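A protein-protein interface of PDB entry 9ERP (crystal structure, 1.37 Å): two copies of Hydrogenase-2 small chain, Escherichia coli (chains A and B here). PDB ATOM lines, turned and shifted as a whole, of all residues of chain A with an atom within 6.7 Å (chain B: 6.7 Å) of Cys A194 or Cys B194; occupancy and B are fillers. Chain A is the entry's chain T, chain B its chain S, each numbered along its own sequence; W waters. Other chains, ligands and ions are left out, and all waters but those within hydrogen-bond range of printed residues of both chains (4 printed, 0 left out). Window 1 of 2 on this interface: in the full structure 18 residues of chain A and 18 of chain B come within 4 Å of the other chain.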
ATOM      1  N   LEU A 189      17.994 -12.514  -7.506  1.00  0.00           N
ATOM      2  CA  LEU A 189      19.379 -12.077  -7.421  1.00  0.00           C
ATOM      3  C   LEU A 189      20.309 -13.111  -8.059  1.00  0.00           C
ATOM      4  O   LEU A 189      20.141 -14.328  -7.921  1.00  0.00           O
ATOM      5  CB  LEU A 189      19.794 -11.896  -5.956  1.00  0.00           C
ATOM      6  CG  LEU A 189      19.156 -10.714  -5.227  1.00  0.00           C
ATOM      7  CD1 LEU A 189      19.411 -10.881  -3.721  1.00  0.00           C
ATOM      8  CD2 LEU A 189      19.684  -9.381  -5.751  1.00  0.00           C
ATOM      9  N   ILE A 190      21.351 -12.629  -8.714  1.00  0.00           N
ATOM     10  CA  ILE A 190      22.325 -13.562  -9.272  1.00  0.00           C
ATOM     11  C   ILE A 190      22.929 -14.449  -8.186  1.00  0.00           C
ATOM     12  O   ILE A 190      23.064 -15.664  -8.360  1.00  0.00           O
ATOM     13  CB  ILE A 190      23.396 -12.781 -10.068  1.00  0.00           C
ATOM     14  CG1 ILE A 190      22.748 -12.208 -11.334  1.00  0.00           C
ATOM     15  CG2 ILE A 190      24.590 -13.658 -10.369  1.00  0.00           C
ATOM     16  CD1 ILE A 190      23.648 -11.172 -12.067  1.00  0.00           C
ATOM     17  N   HIS A 191      23.251 -13.865  -7.029  1.00  0.00           N
ATOM     18  CA  HIS A 191      23.834 -14.598  -5.915  1.00  0.00           C
ATOM     19  C   HIS A 191      22.881 -15.629  -5.330  1.00  0.00           C
ATOM     20  O   HIS A 191      23.352 -16.555  -4.662  1.00  0.00           O
ATOM     21  CB  HIS A 191      24.208 -13.556  -4.865  1.00  0.00           C
ATOM     22  CG  HIS A 191      24.857 -14.092  -3.631  1.00  0.00           C
ATOM     23  ND1 HIS A 191      26.157 -14.547  -3.599  1.00  0.00           N
ATOM     24  CD2 HIS A 191      24.393 -14.180  -2.358  1.00  0.00           C
ATOM     25  CE1 HIS A 191      26.455 -14.918  -2.368  1.00  0.00           C
ATOM     26  NE2 HIS A 191      25.402 -14.697  -1.599  1.00  0.00           N
ATOM     27  N   GLU A 192      21.581 -15.495  -5.557  1.00  0.00           N
ATOM     28  CA  GLU A 192      20.612 -16.489  -5.101  1.00  0.00           C
ATOM     29  C   GLU A 192      20.367 -17.570  -6.132  1.00  0.00           C
ATOM     30  O   GLU A 192      19.440 -18.381  -5.960  1.00  0.00           O
ATOM     31  CB  GLU A 192      19.306 -15.818  -4.676  1.00  0.00           C
ATOM     32  CG  GLU A 192      19.480 -14.961  -3.425  1.00  0.00           C
ATOM     33  CD  GLU A 192      19.992 -15.767  -2.248  1.00  0.00           C
ATOM     34  OE1 GLU A 192      19.399 -16.821  -1.939  1.00  0.00           O
ATOM     35  OE2 GLU A 192      21.022 -15.380  -1.640  1.00  0.00           O
ATOM     36  N   HIS A 193      21.194 -17.614  -7.194  1.00  0.00           N
ATOM     37  CA  HIS A 193      21.154 -18.726  -8.150  1.00  0.00           C
ATOM     38  C   HIS A 193      22.515 -18.866  -8.841  1.00  0.00           C
ATOM     39  O   HIS A 193      22.604 -19.128 -10.050  1.00  0.00           O
ATOM     40  CB  HIS A 193      20.009 -18.565  -9.154  1.00  0.00           C
ATOM     41  CG  HIS A 193      19.442 -19.863  -9.628  1.00  0.00           C
ATOM     42  ND1 HIS A 193      18.167 -20.291  -9.301  1.00  0.00           N
ATOM     43  CD2 HIS A 193      19.982 -20.838 -10.392  1.00  0.00           C
ATOM     44  CE1 HIS A 193      17.957 -21.482  -9.843  1.00  0.00           C
ATOM     45  NE2 HIS A 193      19.041 -21.835 -10.507  1.00  0.00           N
ATOM     46  N   CYS A 194      23.593 -18.719  -8.076  1.00  0.00           N
ATOM     47  CA  CYS A 194      24.959 -18.737  -8.595  1.00  0.00           C
ATOM     48  C   CYS A 194      25.668 -20.027  -8.217  1.00  0.00           C
ATOM     49  O   CYS A 194      25.693 -20.414  -7.036  1.00  0.00           O
ATOM     50  CB  CYS A 194      25.759 -17.567  -8.017  1.00  0.00           C
ATOM     51  SG  CYS A 194      27.465 -17.594  -8.589  1.00  0.00           S
ATOM     52  N   GLU A 195      26.274 -20.685  -9.212  1.00  0.00           N
ATOM     53  CA  GLU A 195      26.922 -21.968  -8.996  1.00  0.00           C
ATOM     54  C   GLU A 195      28.152 -21.890  -8.095  1.00  0.00           C
ATOM     55  O   GLU A 195      28.633 -22.940  -7.661  1.00  0.00           O
ATOM     56  CB  GLU A 195      27.263 -22.628 -10.340  1.00  0.00           C
ATOM     57  CG  GLU A 195      28.434 -21.924 -11.109  1.00  0.00           C
ATOM     58  CD  GLU A 195      27.970 -20.781 -12.011  1.00  0.00           C
ATOM     59  OE1 GLU A 195      26.870 -20.221 -11.796  1.00  0.00           O
ATOM     60  OE2 GLU A 195      28.755 -20.399 -12.909  1.00  0.00           O
ATOM     61  N   ARG A 196      28.666 -20.698  -7.788  1.00  0.00           N
ATOM     62  CA  ARG A 196      29.786 -20.573  -6.852  1.00  0.00           C
ATOM     63  C   ARG A 196      29.339 -20.304  -5.420  1.00  0.00           C
ATOM     64  O   ARG A 196      30.191 -20.136  -4.531  1.00  0.00           O
ATOM     65  CB  ARG A 196      30.767 -19.487  -7.331  1.00  0.00           C
ATOM     66  CG  ARG A 196      31.222 -19.774  -8.761  1.00  0.00           C
ATOM     67  CD  ARG A 196      32.453 -18.991  -9.142  1.00  0.00           C
ATOM     68  NE  ARG A 196      32.897 -19.407 -10.468  1.00  0.00           N
ATOM     69  CZ  ARG A 196      34.096 -19.171 -10.966  1.00  0.00           C
ATOM     70  NH1 ARG A 196      34.993 -18.445 -10.306  1.00  0.00           N
ATOM     71  NH2 ARG A 196      34.415 -19.677 -12.147  1.00  0.00           N
ATOM     72  N   ARG A 197      28.039 -20.282  -5.169  1.00  0.00           N
ATOM     73  CA  ARG A 197      27.571 -20.107  -3.798  1.00  0.00           C
ATOM     74  C   ARG A 197      28.164 -21.119  -2.830  1.00  0.00           C
ATOM     75  O   ARG A 197      28.426 -20.740  -1.679  1.00  0.00           O
ATOM     76  CB  ARG A 197      26.038 -20.147  -3.776  1.00  0.00           C
ATOM     77  CG  ARG A 197      25.396 -19.993  -2.418  1.00  0.00           C
ATOM     78  CD  ARG A 197      25.738 -18.645  -1.770  1.00  0.00           C
ATOM     79  NE  ARG A 197      24.959 -18.488  -0.543  1.00  0.00           N
ATOM     80  CZ  ARG A 197      23.747 -17.961  -0.475  1.00  0.00           C
ATOM     81  NH1 ARG A 197      23.193 -17.341  -1.513  1.00  0.00           N
ATOM     82  NH2 ARG A 197      23.064 -18.060   0.665  1.00  0.00           N
ATOM     83  N   PRO A 198      28.386 -22.381  -3.191  1.00  0.00           N
ATOM     84  CA  PRO A 198      29.035 -23.286  -2.227  1.00  0.00           C
ATOM     85  C   PRO A 198      30.373 -22.762  -1.732  1.00  0.00           C
ATOM     86  O   PRO A 198      30.718 -22.943  -0.550  1.00  0.00           O
ATOM     87  CB  PRO A 198      29.206 -24.589  -3.013  1.00  0.00           C
ATOM     88  CG  PRO A 198      28.128 -24.539  -4.069  1.00  0.00           C
ATOM     89  CD  PRO A 198      28.023 -23.089  -4.443  1.00  0.00           C
ATOM     90  N   CYS A 225      32.468  -8.978  -6.600  1.00  0.00           N
ATOM     91  CA  CYS A 225      31.274  -9.486  -7.262  1.00  0.00           C
ATOM     92  C   CYS A 225      30.020  -8.808  -6.726  1.00  0.00           C
ATOM     93  O   CYS A 225      29.770  -8.780  -5.510  1.00  0.00           O
ATOM     94  CB  CYS A 225      31.187 -10.997  -7.090  1.00  0.00           C
ATOM     95  SG  CYS A 225      29.825 -11.690  -8.079  1.00  0.00           S
ATOM     96  N   SER A 235      23.654 -16.122 -14.450  1.00  0.00           N
ATOM     97  CA  SER A 235      24.219 -17.398 -14.058  1.00  0.00           C
ATOM     98  C   SER A 235      23.473 -18.576 -14.650  1.00  0.00           C
ATOM     99  O   SER A 235      24.056 -19.668 -14.713  1.00  0.00           O
ATOM    100  CB  SER A 235      24.237 -17.537 -12.535  1.00  0.00           C
ATOM    101  OG  SER A 235      22.917 -17.433 -12.050  1.00  0.00           O
ATOM    102  N   THR A 236      22.240 -18.386 -15.118  1.00  0.00           N
ATOM    103  CA  THR A 236      21.422 -19.489 -15.628  1.00  0.00           C
ATOM    104  C   THR A 236      21.356 -19.412 -17.150  1.00  0.00           C
ATOM    105  O   THR A 236      21.920 -20.282 -17.849  1.00  0.00           O
ATOM    106  CB  THR A 236      20.024 -19.535 -15.000  1.00  0.00           C
ATOM    107  OG1 THR A 236      19.418 -18.239 -15.027  1.00  0.00           O
ATOM    108  CG2 THR A 236      20.056 -20.040 -13.557  1.00  0.00           C
ATOM    109  N   TRP A 246      29.451 -16.752 -18.780  1.00  0.00           N
ATOM    110  CA  TRP A 246      29.039 -15.493 -18.177  1.00  0.00           C
ATOM    111  C   TRP A 246      30.233 -14.946 -17.420  1.00  0.00           C
ATOM    112  O   TRP A 246      31.242 -15.641 -17.256  1.00  0.00           O
ATOM    113  CB  TRP A 246      27.804 -15.649 -17.289  1.00  0.00           C
ATOM    114  CG  TRP A 246      27.919 -16.424 -15.970  1.00  0.00           C
ATOM    115  CD1 TRP A 246      28.143 -17.752 -15.805  1.00  0.00           C
ATOM    116  CD2 TRP A 246      27.710 -15.889 -14.656  1.00  0.00           C
ATOM    117  NE1 TRP A 246      28.109 -18.080 -14.467  1.00  0.00           N
ATOM    118  CE2 TRP A 246      27.846 -16.944 -13.748  1.00  0.00           C
ATOM    119  CE3 TRP A 246      27.420 -14.604 -14.167  1.00  0.00           C
ATOM    120  CZ2 TRP A 246      27.692 -16.766 -12.363  1.00  0.00           C
ATOM    121  CZ3 TRP A 246      27.281 -14.436 -12.812  1.00  0.00           C
ATOM    122  CH2 TRP A 246      27.405 -15.518 -11.927  1.00  0.00           C
ATOM    123  N   VAL A 248      31.272 -14.329 -14.350  1.00  0.00           N
ATOM    124  CA  VAL A 248      31.830 -15.051 -13.205  1.00  0.00           C
ATOM    125  C   VAL A 248      32.432 -16.364 -13.661  1.00  0.00           C
ATOM    126  O   VAL A 248      33.515 -16.759 -13.218  1.00  0.00           O
ATOM    127  CB  VAL A 248      30.734 -15.216 -12.126  1.00  0.00           C
ATOM    128  CG1 VAL A 248      31.085 -16.294 -11.141  1.00  0.00           C
ATOM    129  CG2 VAL A 248      30.456 -13.848 -11.422  1.00  0.00           C
ATOM    130  N   LEU B 189      32.525 -32.115  -5.961  1.00  0.00           N
ATOM    131  CA  LEU B 189      31.141 -32.546  -5.834  1.00  0.00           C
ATOM    132  C   LEU B 189      30.217 -31.606  -6.612  1.00  0.00           C
ATOM    133  O   LEU B 189      30.397 -30.384  -6.619  1.00  0.00           O
ATOM    134  CB  LEU B 189      30.705 -32.519  -4.363  1.00  0.00           C
ATOM    135  CG  LEU B 189      31.330 -33.558  -3.436  1.00  0.00           C
ATOM    136  CD1 LEU B 189      31.008 -33.213  -1.968  1.00  0.00           C
ATOM    137  CD2 LEU B 189      30.796 -34.942  -3.784  1.00  0.00           C
ATOM    138  N   ILE B 190      29.200 -32.170  -7.250  1.00  0.00           N
ATOM    139  CA  ILE B 190      28.225 -31.335  -7.949  1.00  0.00           C
ATOM    140  C   ILE B 190      27.614 -30.312  -6.998  1.00  0.00           C
ATOM    141  O   ILE B 190      27.470 -29.137  -7.339  1.00  0.00           O
ATOM    142  CB  ILE B 190      27.157 -32.231  -8.652  1.00  0.00           C
ATOM    143  CG1 ILE B 190      27.815 -32.974  -9.813  1.00  0.00           C
ATOM    144  CG2 ILE B 190      25.972 -31.416  -9.116  1.00  0.00           C
ATOM    145  CD1 ILE B 190      26.963 -34.097 -10.374  1.00  0.00           C
ATOM    146  N   HIS B 191      27.275 -30.737  -5.777  1.00  0.00           N
ATOM    147  CA  HIS B 191      26.669 -29.830  -4.806  1.00  0.00           C
ATOM    148  C   HIS B 191      27.620 -28.714  -4.363  1.00  0.00           C
ATOM    149  O   HIS B 191      27.140 -27.694  -3.851  1.00  0.00           O
ATOM    150  CB  HIS B 191      26.276 -30.702  -3.614  1.00  0.00           C
ATOM    151  CG  HIS B 191      25.591 -29.997  -2.488  1.00  0.00           C
ATOM    152  ND1 HIS B 191      24.277 -29.565  -2.549  1.00  0.00           N
ATOM    153  CD2 HIS B 191      26.034 -29.692  -1.240  1.00  0.00           C
ATOM    154  CE1 HIS B 191      23.943 -29.038  -1.381  1.00  0.00           C
ATOM    155  NE2 HIS B 191      24.989 -29.098  -0.576  1.00  0.00           N
ATOM    156  N   GLU B 192      28.933 -28.889  -4.498  1.00  0.00           N
ATOM    157  CA  GLU B 192      29.883 -27.835  -4.171  1.00  0.00           C
ATOM    158  C   GLU B 192      30.141 -26.908  -5.362  1.00  0.00           C
ATOM    159  O   GLU B 192      31.034 -26.058  -5.299  1.00  0.00           O
ATOM    160  CB  GLU B 192      31.162 -28.460  -3.642  1.00  0.00           C
ATOM    161  CG  GLU B 192      30.968 -29.144  -2.268  1.00  0.00           C
ATOM    162  CD  GLU B 192      30.386 -28.199  -1.241  1.00  0.00           C
ATOM    163  OE1 GLU B 192      30.974 -27.129  -1.047  1.00  0.00           O
ATOM    164  OE2 GLU B 192      29.336 -28.507  -0.612  1.00  0.00           O
ATOM    165  N   HIS B 193      29.328 -27.008  -6.423  1.00  0.00           N
ATOM    166  CA  HIS B 193      29.399 -26.055  -7.541  1.00  0.00           C
ATOM    167  C   HIS B 193      28.050 -26.018  -8.261  1.00  0.00           C
ATOM    168  O   HIS B 193      27.990 -25.926  -9.495  1.00  0.00           O
ATOM    169  CB  HIS B 193      30.563 -26.375  -8.484  1.00  0.00           C
ATOM    170  CG  HIS B 193      31.170 -25.162  -9.127  1.00  0.00           C
ATOM    171  ND1 HIS B 193      32.439 -24.697  -8.826  1.00  0.00           N
ATOM    172  CD2 HIS B 193      30.665 -24.308 -10.034  1.00  0.00           C
ATOM    173  CE1 HIS B 193      32.692 -23.626  -9.558  1.00  0.00           C
ATOM    174  NE2 HIS B 193      31.622 -23.358 -10.285  1.00  0.00           N
ATOM    175  N   CYS B 194      26.959 -26.062  -7.500  1.00  0.00           N
ATOM    176  CA  CYS B 194      25.613 -26.107  -8.048  1.00  0.00           C
ATOM    177  C   CYS B 194      24.914 -24.765  -7.863  1.00  0.00           C
ATOM    178  O   CYS B 194      24.916 -24.192  -6.756  1.00  0.00           O
ATOM    179  CB  CYS B 194      24.780 -27.184  -7.353  1.00  0.00           C
ATOM    180  SG  CYS B 194      23.060 -27.242  -7.935  1.00  0.00           S
ATOM    181  N   GLU B 195      24.280 -24.275  -8.931  1.00  0.00           N
ATOM    182  CA  GLU B 195      23.636 -22.960  -8.904  1.00  0.00           C
ATOM    183  C   GLU B 195      22.375 -22.918  -8.058  1.00  0.00           C
ATOM    184  O   GLU B 195      21.841 -21.815  -7.824  1.00  0.00           O
ATOM    185  CB  GLU B 195      23.347 -22.495 -10.345  1.00  0.00           C
ATOM    186  CG  GLU B 195      22.233 -23.261 -11.097  1.00  0.00           C
ATOM    187  CD  GLU B 195      22.671 -24.548 -11.814  1.00  0.00           C
ATOM    188  OE1 GLU B 195      23.762 -25.104 -11.540  1.00  0.00           O
ATOM    189  OE2 GLU B 195      21.883 -25.020 -12.699  1.00  0.00           O
ATOM    190  N   ARG B 196      21.889 -24.077  -7.589  1.00  0.00           N
ATOM    191  CA  ARG B 196      20.754 -24.082  -6.691  1.00  0.00           C
ATOM    192  C   ARG B 196      21.175 -24.122  -5.237  1.00  0.00           C
ATOM    193  O   ARG B 196      20.306 -24.155  -4.351  1.00  0.00           O
ATOM    194  CB  ARG B 196      19.807 -25.238  -7.026  1.00  0.00           C
ATOM    195  CG  ARG B 196      19.326 -25.129  -8.478  1.00  0.00           C
ATOM    196  CD  ARG B 196      18.102 -25.943  -8.785  1.00  0.00           C
ATOM    197  NE  ARG B 196      17.713 -25.713 -10.173  1.00  0.00           N
ATOM    198  CZ  ARG B 196      16.526 -26.006 -10.672  1.00  0.00           C
ATOM    199  NH1 ARG B 196      15.613 -26.624  -9.946  1.00  0.00           N
ATOM    200  NH2 ARG B 196      16.261 -25.704 -11.937  1.00  0.00           N
ATOM    201  N   ARG B 197      22.471 -24.066  -4.964  1.00  0.00           N
ATOM    202  CA  ARG B 197      22.913 -24.055  -3.571  1.00  0.00           C
ATOM    203  C   ARG B 197      22.301 -22.918  -2.764  1.00  0.00           C
ATOM    204  O   ARG B 197      22.001 -23.143  -1.577  1.00  0.00           O
ATOM    205  CB  ARG B 197      24.441 -23.995  -3.530  1.00  0.00           C
ATOM    206  CG  ARG B 197      25.022 -23.968  -2.115  1.00  0.00           C
ATOM    207  CD  ARG B 197      24.696 -25.241  -1.316  1.00  0.00           C
ATOM    208  NE  ARG B 197      25.416 -25.213  -0.050  1.00  0.00           N
ATOM    209  CZ  ARG B 197      26.639 -25.700   0.132  1.00  0.00           C
ATOM    210  NH1 ARG B 197      27.252 -26.404  -0.803  1.00  0.00           N
ATOM    211  NH2 ARG B 197      27.282 -25.437   1.271  1.00  0.00           N
ATOM    212  N   PRO B 198      22.090 -21.704  -3.299  1.00  0.00           N
ATOM    213  CA  PRO B 198      21.429 -20.685  -2.470  1.00  0.00           C
ATOM    214  C   PRO B 198      20.069 -21.138  -1.951  1.00  0.00           C
ATOM    215  O   PRO B 198      19.692 -20.796  -0.821  1.00  0.00           O
ATOM    216  CB  PRO B 198      21.279 -19.485  -3.415  1.00  0.00           C
ATOM    217  CG  PRO B 198      22.369 -19.686  -4.448  1.00  0.00           C
ATOM    218  CD  PRO B 198      22.442 -21.181  -4.632  1.00  0.00           C
ATOM    219  N   CYS B 225      17.995 -35.451  -4.872  1.00  0.00           N
ATOM    220  CA  CYS B 225      19.205 -35.042  -5.554  1.00  0.00           C
ATOM    221  C   CYS B 225      20.460 -35.631  -4.912  1.00  0.00           C
ATOM    222  O   CYS B 225      20.694 -35.492  -3.703  1.00  0.00           O
ATOM    223  CB  CYS B 225      19.286 -33.516  -5.582  1.00  0.00           C
ATOM    224  SG  CYS B 225      20.665 -32.974  -6.614  1.00  0.00           S
ATOM    225  N   SER B 235      27.049 -29.541 -13.459  1.00  0.00           N
ATOM    226  CA  SER B 235      26.456 -28.229 -13.257  1.00  0.00           C
ATOM    227  C   SER B 235      27.196 -27.136 -14.001  1.00  0.00           C
ATOM    228  O   SER B 235      26.621 -26.069 -14.201  1.00  0.00           O
ATOM    229  CB  SER B 235      26.405 -27.876 -11.763  1.00  0.00           C
ATOM    230  OG  SER B 235      27.730 -27.876 -11.257  1.00  0.00           O
ATOM    231  N   THR B 236      28.441 -27.370 -14.404  1.00  0.00           N
ATOM    232  CA  THR B 236      29.266 -26.367 -15.056  1.00  0.00           C
ATOM    233  C   THR B 236      29.401 -26.659 -16.543  1.00  0.00           C
ATOM    234  O   THR B 236      28.910 -25.886 -17.369  1.00  0.00           O
ATOM    235  CB  THR B 236      30.661 -26.245 -14.406  1.00  0.00           C
ATOM    236  OG1 THR B 236      31.258 -27.530 -14.235  1.00  0.00           O
ATOM    237  CG2 THR B 236      30.549 -25.548 -13.041  1.00  0.00           C
ATOM    238  N   TRP B 246      21.327 -29.534 -17.939  1.00  0.00           N
ATOM    239  CA  TRP B 246      21.717 -30.693 -17.148  1.00  0.00           C
ATOM    240  C   TRP B 246      20.501 -31.129 -16.359  1.00  0.00           C
ATOM    241  O   TRP B 246      19.478 -30.431 -16.346  1.00  0.00           O
ATOM    242  CB  TRP B 246      22.933 -30.385 -16.262  1.00  0.00           C
ATOM    243  CG  TRP B 246      22.790 -29.474 -15.081  1.00  0.00           C
ATOM    244  CD1 TRP B 246      22.601 -28.111 -15.098  1.00  0.00           C
ATOM    245  CD2 TRP B 246      22.962 -29.835 -13.700  1.00  0.00           C
ATOM    246  NE1 TRP B 246      22.614 -27.622 -13.812  1.00  0.00           N
ATOM    247  CE2 TRP B 246      22.852 -28.649 -12.945  1.00  0.00           C
ATOM    248  CE3 TRP B 246      23.244 -31.040 -13.033  1.00  0.00           C
ATOM    249  CZ2 TRP B 246      22.956 -28.641 -11.540  1.00  0.00           C
ATOM    250  CZ3 TRP B 246      23.369 -31.032 -11.652  1.00  0.00           C
ATOM    251  CH2 TRP B 246      23.231 -29.831 -10.931  1.00  0.00           C
ATOM    252  N   VAL B 248      19.375 -31.301 -13.254  1.00  0.00           N
ATOM    253  CA  VAL B 248      18.792 -30.426 -12.246  1.00  0.00           C
ATOM    254  C   VAL B 248      18.199 -29.187 -12.899  1.00  0.00           C
ATOM    255  O   VAL B 248      17.096 -28.747 -12.559  1.00  0.00           O
ATOM    256  CB  VAL B 248      19.857 -30.102 -11.191  1.00  0.00           C
ATOM    257  CG1 VAL B 248      19.435 -28.888 -10.381  1.00  0.00           C
ATOM    258  CG2 VAL B 248      20.095 -31.318 -10.287  1.00  0.00           C
HETATM  259  O   HOH W   1      31.390 -21.225 -12.285  1.00  0.00           O
HETATM  260  O   HOH W   2      30.215 -25.400   0.805  1.00  0.00           O
HETATM  261  O   HOH W   3      19.320 -24.236 -12.188  1.00  0.00           O
HETATM  262  O   HOH W   4      20.198 -18.210   0.234  1.00  0.00           O
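The side-chain carboxylate of Glu B195 lies within hydrogen-bond range of the indole nitrogen of Trp B246, at 2.9 Å.
The side-chain sulfur (SG) of Cys A194 lies close to the backbone NH (N) of Arg A196, at 3.4 Å.
O of His A191 sits at hydrogen-bond distance from NH1 of Arg A197 (3.2 Å).
The side-chain carboxylate (OE2) of Glu A195 sits at hydrogen-bond distance from the indole nitrogen (NE1) of Trp A246.
OG of Ser A235 sits at hydrogen-bond distance from O of His A193 (2.6 Å).
OE2 of Glu A192 is in salt-bridge range of NH1 of Arg A197 (2.9 Å).
His A191 touches Pro B198.
Glu B195 touches His A193 (O to CA, 3.2 Å).
O of Cys A194 touches O of Cys B194 (3.9 Å).
N of Cys A194 touches O of Glu B195 (3.6 Å).
N of Cys A194 touches CG of Pro B198, at 3.9 Å.
Glu A195 touches Cys B194.
Arg A197 touches Pro B198.
Pro A198 touches His B191.
Glu B192 touches Pro A198.
Pro A198 touches Arg B197.
Of the printed residues of chain B, His A193 touches Glu B195, Arg B196 and Pro B198.
Printed residues of chain A within 4 Å of Cys B194: Cys A194, Glu A195 and Pro A198.
Of the printed residues of chain A, Arg B196 touches His A193.
Of the printed residues of chain A, Arg B197 touches Pro A198 (3.5 Å).
Of the printed residues of chain A, Pro B198 touches His A191, Glu A192, His A193, Cys A194 and Arg A197.
Trp B246 touches none of the printed residues of chain A.
Val B248 touches none of the printed residues of chain A.
The nearest residue of chain A that does not touch Cys B194 is Arg A197 (5.1 Å).
Of the 15 printed residues of chain B, 8 touch a printed residue of chain A.
Of the 15 printed residues of chain A, 8 touch a printed residue of chain B.
Printed residues of chain A that touch a printed residue of chain B: His A191, Glu A192, His A193, Cys A194, Glu A195, Arg A196, Arg A197 and Pro A198.
Among the printed residues, no Asp or Glu carboxylate lies within 4 Å of a Lys or Arg side-chain nitrogen of the other chain.
His A193 touches Arg B196, and with the chains exchanged Arg A196 touches His B193.
His A193 touches Pro B198, and with the chains exchanged Pro A198 touches His B193.
Cys A194 touches Pro B198, and with the chains exchanged Pro A198 touches Cys B194.
Arg A197 touches Pro B198, and with the chains exchanged Pro A198 touches Arg B197.
Positions printed for both chains: 189, 190, 191, 192, 193, 194, 195, 196, 197, 198, 225, 235, 236, 246 and 248.
Water W2 lies within hydrogen-bond range of OE1 of Glu B192, O of Pro A198 and NH2 of Arg B197.
Water W4 lies within hydrogen-bond range of OE1 of Glu A192 (2.7 Å), O of Pro B198 (2.8 Å) and NH2 of Arg A197 (2.9 Å).
Water W3 lies within hydrogen-bond range of the side-chain carboxylate of Glu B195 (2.7 Å), a ring nitrogen (NE2) of His A193 (2.9 Å) and the guanidinium group of Arg B196 (3.0 Å).
Water W1 lies within hydrogen-bond range of OE2 of Glu A195 (2.8 Å), NE2 of His B193 (2.9 Å) and NE of Arg A196 (3.0 Å).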
